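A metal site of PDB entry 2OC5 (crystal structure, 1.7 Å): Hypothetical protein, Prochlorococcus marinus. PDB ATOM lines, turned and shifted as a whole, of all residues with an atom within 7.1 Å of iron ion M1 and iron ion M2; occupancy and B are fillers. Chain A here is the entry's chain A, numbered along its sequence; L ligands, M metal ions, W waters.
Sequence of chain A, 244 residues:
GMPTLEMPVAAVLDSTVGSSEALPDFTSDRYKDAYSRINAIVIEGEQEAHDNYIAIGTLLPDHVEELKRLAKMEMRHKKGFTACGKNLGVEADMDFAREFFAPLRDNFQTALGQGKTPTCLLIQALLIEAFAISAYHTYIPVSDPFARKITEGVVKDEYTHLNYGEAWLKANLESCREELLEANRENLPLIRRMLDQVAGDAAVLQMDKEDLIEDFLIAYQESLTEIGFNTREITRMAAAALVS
Iron ion M2 is bound by water W1, the side-chain carboxylate (OE2) of Glu 74, the side-chain carboxylate (OE2) of Glu 129, an oxygen (O3) of the ligand, the side-chain carboxylate (OE1) of Glu 129 and a ring nitrogen (ND1) of His 161. Iron ion M2 has six donor atoms within binding distance.
Glu 158 touches iron ion M1 (OE1 to FE, 3.6 Å). The nearest printed residue that does not touch iron ion M1 is His 161 (4.6 Å).
Water W2 bridges OE2 of Glu 158 (2.5 Å) and OE2 of Glu 46 (2.6 Å).
Water W1 binds iron ion M1, at 1.9 Å. The side-chain carboxylate (OE1) of Glu 74 is bound to iron ion M1 (2.0 Å). Water W2 is bound to iron ion M1 (2.0 Å). The side-chain carboxylate (OE1) of Glu 46 binds iron ion M1 (2.1 Å). Iron ion M1 is bound by an oxygen (O1) of the ligand, 2.1 Å away. A ring nitrogen (ND1) of His 77 is bound to iron ion M1 (2.2 Å).
OH of Tyr 136 is in hydrogen-bond range of OE2 of Glu 46, 2.7 Å away. A ring nitrogen (NE2) of His 77 sits at hydrogen-bond distance from the side-chain carboxylate (OD2) of Asp 157 (2.7 Å). N of Glu 129 sits at hydrogen-bond distance from O of Gln 124. The side-chain carboxylate (OE2) of Glu 129 sits close to the side-chain hydroxyl (OH) of Tyr 53, 2.6 Å away. A ring nitrogen (NE2) of His 161 sits at hydrogen-bond distance from the side-chain sulfur (SD) of Met 73 (3.4 Å).
Glu 158 touches iron ion M2. Four residues have an atom within 4 Å of iron ion M2: Glu 74, Glu 129, Glu 158 and His 161. Along chain A the residues within 4 Å of iron ion M2 span positions 74 to 161.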
ATOM      1  N   VAL A  42      12.035 -22.571  17.486  1.00  0.00           N
ATOM      2  CA  VAL A  42      11.896 -21.428  16.621  1.00  0.00           C
ATOM      3  C   VAL A  42      12.861 -21.532  15.388  1.00  0.00           C
ATOM      4  O   VAL A  42      12.453 -21.346  14.235  1.00  0.00           O
ATOM      5  CB  VAL A  42      12.181 -20.165  17.475  1.00  0.00           C
ATOM      6  CG1 VAL A  42      12.392 -18.958  16.633  1.00  0.00           C
ATOM      7  CG2 VAL A  42      10.985 -19.949  18.483  1.00  0.00           C
ATOM      8  N   GLY A  45      11.531 -24.173  13.128  1.00  0.00           N
ATOM      9  CA  GLY A  45      10.336 -23.654  12.507  1.00  0.00           C
ATOM     10  C   GLY A  45      10.614 -22.716  11.347  1.00  0.00           C
ATOM     11  O   GLY A  45       9.970 -22.822  10.295  1.00  0.00           O
ATOM     12  N   GLU A  46      11.542 -21.799  11.539  1.00  0.00           N
ATOM     13  CA  GLU A  46      11.937 -20.882  10.459  1.00  0.00           C
ATOM     14  C   GLU A  46      12.543 -21.636   9.250  1.00  0.00           C
ATOM     15  O   GLU A  46      12.194 -21.370   8.107  1.00  0.00           O
ATOM     16  CB  GLU A  46      12.882 -19.773  10.964  1.00  0.00           C
ATOM     17  CG  GLU A  46      12.404 -18.973  12.178  1.00  0.00           C
ATOM     18  CD  GLU A  46      11.228 -18.051  11.958  1.00  0.00           C
ATOM     19  OE1 GLU A  46      10.913 -17.819  10.802  1.00  0.00           O
ATOM     20  OE2 GLU A  46      10.629 -17.542  12.969  1.00  0.00           O
ATOM     21  N   ALA A  49       9.715 -23.423   7.476  1.00  0.00           N
ATOM     22  CA  ALA A  49       8.906 -22.433   6.769  1.00  0.00           C
ATOM     23  C   ALA A  49       9.560 -22.086   5.432  1.00  0.00           C
ATOM     24  O   ALA A  49       8.875 -22.064   4.389  1.00  0.00           O
ATOM     25  CB  ALA A  49       8.759 -21.214   7.644  1.00  0.00           C
ATOM     26  N   HIS A  50      10.874 -21.793   5.444  1.00  0.00           N
ATOM     27  CA  HIS A  50      11.622 -21.685   4.209  1.00  0.00           C
ATOM     28  C   HIS A  50      11.371 -22.833   3.253  1.00  0.00           C
ATOM     29  O   HIS A  50      11.043 -22.626   2.056  1.00  0.00           O
ATOM     30  CB  HIS A  50      13.127 -21.561   4.488  1.00  0.00           C
ATOM     31  CG  HIS A  50      13.979 -21.735   3.275  1.00  0.00           C
ATOM     32  ND1 HIS A  50      14.314 -22.984   2.781  1.00  0.00           N
ATOM     33  CD2 HIS A  50      14.526 -20.833   2.414  1.00  0.00           C
ATOM     34  CE1 HIS A  50      15.051 -22.828   1.690  1.00  0.00           C
ATOM     35  NE2 HIS A  50      15.170 -21.526   1.434  1.00  0.00           N
ATOM     36  N   TYR A  53       7.684 -22.894   1.831  1.00  0.00           N
ATOM     37  CA  TYR A  53       7.321 -21.922   0.789  1.00  0.00           C
ATOM     38  C   TYR A  53       7.968 -22.300  -0.546  1.00  0.00           C
ATOM     39  O   TYR A  53       7.316 -22.242  -1.597  1.00  0.00           O
ATOM     40  CB  TYR A  53       7.647 -20.456   1.266  1.00  0.00           C
ATOM     41  CG  TYR A  53       6.615 -19.938   2.304  1.00  0.00           C
ATOM     42  CD1 TYR A  53       5.242 -19.947   2.011  1.00  0.00           C
ATOM     43  CD2 TYR A  53       7.000 -19.474   3.570  1.00  0.00           C
ATOM     44  CE1 TYR A  53       4.280 -19.528   2.959  1.00  0.00           C
ATOM     45  CE2 TYR A  53       6.072 -19.065   4.518  1.00  0.00           C
ATOM     46  CZ  TYR A  53       4.691 -19.080   4.221  1.00  0.00           C
ATOM     47  OH  TYR A  53       3.796 -18.679   5.194  1.00  0.00           O
ATOM     48  N   LEU A  70       9.379 -14.843   0.240  1.00  0.00           N
ATOM     49  CA  LEU A  70       8.902 -15.253   1.585  1.00  0.00           C
ATOM     50  C   LEU A  70       9.940 -16.192   2.237  1.00  0.00           C
ATOM     51  O   LEU A  70      10.300 -16.001   3.411  1.00  0.00           O
ATOM     52  CB  LEU A  70       7.514 -15.924   1.552  1.00  0.00           C
ATOM     53  CG  LEU A  70       6.367 -15.124   0.951  1.00  0.00           C
ATOM     54  CD1 LEU A  70       5.041 -15.838   1.069  1.00  0.00           C
ATOM     55  CD2 LEU A  70       6.293 -13.690   1.496  1.00  0.00           C
ATOM     56  N   MET A  73      12.879 -14.373   3.582  1.00  0.00           N
ATOM     57  CA  MET A  73      12.538 -13.765   4.887  1.00  0.00           C
ATOM     58  C   MET A  73      12.698 -14.790   6.011  1.00  0.00           C
ATOM     59  O   MET A  73      13.181 -14.448   7.097  1.00  0.00           O
ATOM     60  CB  MET A  73      11.118 -13.228   4.913  1.00  0.00           C
ATOM     61  CG  MET A  73      10.873 -12.127   3.933  1.00  0.00           C
ATOM     62  SD  MET A  73       8.955 -11.428   4.098  1.00  0.00           S
ATOM     63  CE  MET A  73       8.754 -10.893   2.121  1.00  0.00           C
ATOM     64  N   GLU A  74      12.236 -16.013   5.790  1.00  0.00           N
ATOM     65  CA  GLU A  74      12.325 -17.046   6.837  1.00  0.00           C
ATOM     66  C   GLU A  74      13.776 -17.310   7.209  1.00  0.00           C
ATOM     67  O   GLU A  74      14.093 -17.517   8.379  1.00  0.00           O
ATOM     68  CB  GLU A  74      11.659 -18.322   6.405  1.00  0.00           C
ATOM     69  CG  GLU A  74      10.147 -18.216   6.071  1.00  0.00           C
ATOM     70  CD  GLU A  74       9.255 -17.855   7.221  1.00  0.00           C
ATOM     71  OE1 GLU A  74       9.738 -17.585   8.347  1.00  0.00           O
ATOM     72  OE2 GLU A  74       8.025 -17.855   6.997  1.00  0.00           O
ATOM     73  N   MET A  75      14.673 -17.307   6.235  1.00  0.00           N
ATOM     74  CA  MET A  75      16.097 -17.514   6.541  1.00  0.00           C
ATOM     75  C   MET A  75      16.693 -16.380   7.346  1.00  0.00           C
ATOM     76  O   MET A  75      17.548 -16.599   8.203  1.00  0.00           O
ATOM     77  CB  MET A  75      16.912 -17.792   5.284  1.00  0.00           C
ATOM     78  CG  MET A  75      16.528 -19.108   4.614  1.00  0.00           C
ATOM     79  SD  MET A  75      16.557 -20.746   5.746  1.00  0.00           S
ATOM     80  CE  MET A  75      18.470 -20.702   6.009  1.00  0.00           C
ATOM     81  N   HIS A  77      14.853 -14.635   9.464  1.00  0.00           N
ATOM     82  CA  HIS A  77      14.288 -14.907  10.791  1.00  0.00           C
ATOM     83  C   HIS A  77      15.180 -15.966  11.509  1.00  0.00           C
ATOM     84  O   HIS A  77      15.528 -15.814  12.682  1.00  0.00           O
ATOM     85  CB  HIS A  77      12.839 -15.454  10.736  1.00  0.00           C
ATOM     86  CG  HIS A  77      11.851 -14.547  10.063  1.00  0.00           C
ATOM     87  ND1 HIS A  77      10.561 -14.958   9.719  1.00  0.00           N
ATOM     88  CD2 HIS A  77      11.941 -13.234   9.750  1.00  0.00           C
ATOM     89  CE1 HIS A  77       9.925 -13.914   9.182  1.00  0.00           C
ATOM     90  NE2 HIS A  77      10.749 -12.863   9.185  1.00  0.00           N
ATOM     91  N   LYS A  78      15.515 -17.040  10.789  1.00  0.00           N
ATOM     92  CA  LYS A  78      16.313 -18.128  11.355  1.00  0.00           C
ATOM     93  C   LYS A  78      17.642 -17.611  11.851  1.00  0.00           C
ATOM     94  O   LYS A  78      18.097 -17.977  12.956  1.00  0.00           O
ATOM     95  CB  LYS A  78      16.539 -19.220  10.312  1.00  0.00           C
ATOM     96  CG  LYS A  78      17.172 -20.470  10.893  1.00  0.00           C
ATOM     97  CD  LYS A  78      17.727 -21.401   9.794  1.00  0.00           C
ATOM     98  CE  LYS A  78      18.263 -22.714  10.450  1.00  0.00           C
ATOM     99  NZ  LYS A  78      18.966 -23.575   9.455  1.00  0.00           N
ATOM    100  N   PHE A  81      17.101 -15.493  15.159  1.00  0.00           N
ATOM    101  CA  PHE A  81      16.810 -16.294  16.339  1.00  0.00           C
ATOM    102  C   PHE A  81      17.997 -17.172  16.761  1.00  0.00           C
ATOM    103  O   PHE A  81      18.195 -17.416  17.923  1.00  0.00           O
ATOM    104  CB  PHE A  81      15.522 -17.096  16.155  1.00  0.00           C
ATOM    105  CG  PHE A  81      14.295 -16.220  16.075  1.00  0.00           C
ATOM    106  CD1 PHE A  81      14.024 -15.276  17.095  1.00  0.00           C
ATOM    107  CD2 PHE A  81      13.382 -16.334  15.049  1.00  0.00           C
ATOM    108  CE1 PHE A  81      12.878 -14.501  17.065  1.00  0.00           C
ATOM    109  CE2 PHE A  81      12.223 -15.545  15.025  1.00  0.00           C
ATOM    110  CZ  PHE A  81      12.004 -14.611  16.015  1.00  0.00           C
ATOM    111  N   GLN A 124       0.945 -24.186   6.570  1.00  0.00           N
ATOM    112  CA  GLN A 124       2.057 -23.222   6.720  1.00  0.00           C
ATOM    113  C   GLN A 124       1.589 -21.787   6.897  1.00  0.00           C
ATOM    114  O   GLN A 124       1.955 -21.122   7.866  1.00  0.00           O
ATOM    115  CB  GLN A 124       3.058 -23.295   5.570  1.00  0.00           C
ATOM    116  CG  GLN A 124       4.197 -22.223   5.659  1.00  0.00           C
ATOM    117  CD  GLN A 124       5.068 -22.283   6.915  1.00  0.00           C
ATOM    118  OE1 GLN A 124       5.559 -23.346   7.261  1.00  0.00           O
ATOM    119  NE2 GLN A 124       5.203 -21.126   7.644  1.00  0.00           N
ATOM    120  N   ILE A 128       0.602 -22.293  11.134  1.00  0.00           N
ATOM    121  CA  ILE A 128       1.948 -22.069  11.650  1.00  0.00           C
ATOM    122  C   ILE A 128       2.247 -20.567  11.791  1.00  0.00           C
ATOM    123  O   ILE A 128       2.821 -20.170  12.774  1.00  0.00           O
ATOM    124  CB  ILE A 128       3.038 -22.849  10.870  1.00  0.00           C
ATOM    125  CG1 ILE A 128       2.856 -24.370  11.057  1.00  0.00           C
ATOM    126  CG2 ILE A 128       4.431 -22.479  11.386  1.00  0.00           C
ATOM    127  CD1 ILE A 128       3.612 -25.248  10.016  1.00  0.00           C
ATOM    128  N   GLU A 129       1.852 -19.771  10.828  1.00  0.00           N
ATOM    129  CA  GLU A 129       2.061 -18.305  10.955  1.00  0.00           C
ATOM    130  C   GLU A 129       1.288 -17.751  12.156  1.00  0.00           C
ATOM    131  O   GLU A 129       1.813 -16.912  12.883  1.00  0.00           O
ATOM    132  CB  GLU A 129       1.718 -17.565   9.677  1.00  0.00           C
ATOM    133  CG  GLU A 129       2.546 -17.934   8.393  1.00  0.00           C
ATOM    134  CD  GLU A 129       4.053 -17.618   8.444  1.00  0.00           C
ATOM    135  OE1 GLU A 129       4.516 -16.866   9.353  1.00  0.00           O
ATOM    136  OE2 GLU A 129       4.720 -18.089   7.503  1.00  0.00           O
ATOM    137  N   ALA A 132       3.191 -18.772  15.303  1.00  0.00           N
ATOM    138  CA  ALA A 132       4.387 -17.938  15.441  1.00  0.00           C
ATOM    139  C   ALA A 132       4.087 -16.537  15.924  1.00  0.00           C
ATOM    140  O   ALA A 132       4.716 -16.001  16.834  1.00  0.00           O
ATOM    141  CB  ALA A 132       5.132 -17.872  14.123  1.00  0.00           C
ATOM    142  N   TYR A 136       5.496 -15.012  19.346  1.00  0.00           N
ATOM    143  CA  TYR A 136       6.376 -13.819  19.268  1.00  0.00           C
ATOM    144  C   TYR A 136       5.749 -12.609  19.998  1.00  0.00           C
ATOM    145  O   TYR A 136       6.439 -11.913  20.755  1.00  0.00           O
ATOM    146  CB  TYR A 136       6.852 -13.490  17.839  1.00  0.00           C
ATOM    147  CG  TYR A 136       7.662 -14.609  17.173  1.00  0.00           C
ATOM    148  CD1 TYR A 136       8.286 -15.573  17.953  1.00  0.00           C
ATOM    149  CD2 TYR A 136       7.690 -14.772  15.843  1.00  0.00           C
ATOM    150  CE1 TYR A 136       8.964 -16.605  17.405  1.00  0.00           C
ATOM    151  CE2 TYR A 136       8.366 -15.840  15.274  1.00  0.00           C
ATOM    152  CZ  TYR A 136       8.990 -16.747  16.052  1.00  0.00           C
ATOM    153  OH  TYR A 136       9.712 -17.825  15.509  1.00  0.00           O
ATOM    154  N   VAL A 154      10.610  -9.293  13.294  1.00  0.00           N
ATOM    155  CA  VAL A 154       9.964 -10.429  12.665  1.00  0.00           C
ATOM    156  C   VAL A 154       8.405 -10.396  12.584  1.00  0.00           C
ATOM    157  O   VAL A 154       7.797 -10.987  11.682  1.00  0.00           O
ATOM    158  CB  VAL A 154      10.420 -11.667  13.478  1.00  0.00           C
ATOM    159  CG1 VAL A 154       9.597 -12.916  13.184  1.00  0.00           C
ATOM    160  CG2 VAL A 154      11.918 -11.918  13.280  1.00  0.00           C
ATOM    161  N   ASP A 157       6.595  -9.337   9.419  1.00  0.00           N
ATOM    162  CA  ASP A 157       6.699 -10.310   8.327  1.00  0.00           C
ATOM    163  C   ASP A 157       5.663 -11.443   8.457  1.00  0.00           C
ATOM    164  O   ASP A 157       5.208 -12.000   7.439  1.00  0.00           O
ATOM    165  CB  ASP A 157       8.080 -10.963   8.320  1.00  0.00           C
ATOM    166  CG  ASP A 157       9.185 -10.033   7.816  1.00  0.00           C
ATOM    167  OD1 ASP A 157       8.869  -8.931   7.315  1.00  0.00           O
ATOM    168  OD2 ASP A 157      10.368 -10.457   7.915  1.00  0.00           O
ATOM    169  N   GLU A 158       5.318 -11.828   9.690  1.00  0.00           N
ATOM    170  CA  GLU A 158       4.312 -12.892   9.936  1.00  0.00           C
ATOM    171  C   GLU A 158       2.990 -12.474   9.304  1.00  0.00           C
ATOM    172  O   GLU A 158       2.317 -13.262   8.673  1.00  0.00           O
ATOM    173  CB  GLU A 158       4.082 -13.155  11.426  1.00  0.00           C
ATOM    174  CG  GLU A 158       5.342 -13.244  12.272  1.00  0.00           C
ATOM    175  CD  GLU A 158       6.297 -14.285  11.795  1.00  0.00           C
ATOM    176  OE1 GLU A 158       6.791 -14.170  10.657  1.00  0.00           O
ATOM    177  OE2 GLU A 158       6.560 -15.249  12.541  1.00  0.00           O
ATOM    178  N   HIS A 161       3.037 -12.970   5.678  1.00  0.00           N
ATOM    179  CA  HIS A 161       2.877 -14.419   5.336  1.00  0.00           C
ATOM    180  C   HIS A 161       1.437 -14.869   5.491  1.00  0.00           C
ATOM    181  O   HIS A 161       0.875 -15.523   4.608  1.00  0.00           O
ATOM    182  CB  HIS A 161       3.803 -15.276   6.167  1.00  0.00           C
ATOM    183  CG  HIS A 161       5.243 -14.962   5.922  1.00  0.00           C
ATOM    184  ND1 HIS A 161       6.257 -15.479   6.684  1.00  0.00           N
ATOM    185  CD2 HIS A 161       5.809 -14.054   5.091  1.00  0.00           C
ATOM    186  CE1 HIS A 161       7.417 -15.008   6.242  1.00  0.00           C
ATOM    187  NE2 HIS A 161       7.169 -14.113   5.306  1.00  0.00           N
ATOM    188  N   LEU A 162       0.835 -14.543   6.630  1.00  0.00           N
ATOM    189  CA  LEU A 162      -0.593 -14.776   6.806  1.00  0.00           C
ATOM    190  C   LEU A 162      -1.439 -14.183   5.676  1.00  0.00           C
ATOM    191  O   LEU A 162      -2.313 -14.837   5.130  1.00  0.00           O
ATOM    192  CB  LEU A 162      -1.050 -14.130   8.099  1.00  0.00           C
ATOM    193  CG  LEU A 162      -0.828 -14.839   9.406  1.00  0.00           C
ATOM    194  CD1 LEU A 162      -1.042 -13.754  10.460  1.00  0.00           C
ATOM    195  CD2 LEU A 162      -1.842 -15.997   9.619  1.00  0.00           C
HETATM  196  O1  LIG L   1       8.398 -18.546  10.825  1.00  0.00           O
HETATM  197  O2  LIG L   1       7.416 -19.196  10.589  1.00  0.00           O
HETATM  198  O3  LIG L   1       6.699 -18.959   9.617  1.00  0.00           O
HETATM  199  O4  LIG L   1       7.096 -20.328  11.524  1.00  0.00           O
HETATM  200  O5  LIG L   1       7.940 -20.450  12.763  1.00  0.00           O
HETATM  201  C1  LIG L   1       7.311 -21.411  13.761  1.00  0.00           C
HETATM  202  C2  LIG L   1       7.807 -21.173  15.176  1.00  0.00           C
HETATM  203  C3  LIG L   1       6.811 -21.647  16.233  1.00  0.00           C
HETATM  204  O6  LIG L   1       7.344 -21.305  17.622  1.00  0.00           O
HETATM  205  O7  LIG L   1       6.528 -21.925  18.758  1.00  0.00           O
HETATM  206  O8  LIG L   1       7.322 -21.924  20.070  1.00  0.00           O
HETATM  207  O9  LIG L   1       6.628 -21.225  21.242  1.00  0.00           O
HETATM  208  O10 LIG L   1       7.501 -20.256  22.075  1.00  0.00           O
HETATM  209  O11 LIG L   1       8.434 -19.360  21.284  1.00  0.00           O
HETATM  210  O12 LIG L   1       8.789 -18.046  21.960  1.00  0.00           O
HETATM  211  O13 LIG L   1       9.646 -17.166  21.064  1.00  0.00           O
HETATM  212  O14 LIG L   1      11.123 -17.319  21.399  1.00  0.00           O
HETATM  213  O15 LIG L   1      11.933 -16.556  20.356  1.00  0.00           O
HETATM  214  O16 LIG L   1      13.422 -16.682  20.616  1.00  0.00           O
HETATM  215  O17 LIG L   1      14.055 -17.927  20.100  1.00  0.00           O
HETATM  216 FE    FE M   1       9.259 -16.754  10.094  1.00  0.00          FE
HETATM  217 FE    FE M   2       6.565 -17.102   8.334  1.00  0.00          FE
HETATM  218  O   HOH W   1       7.728 -15.823   9.366  1.00  0.00           O
HETATM  219  O   HOH W   2       8.916 -15.942  11.890  1.00  0.00           O
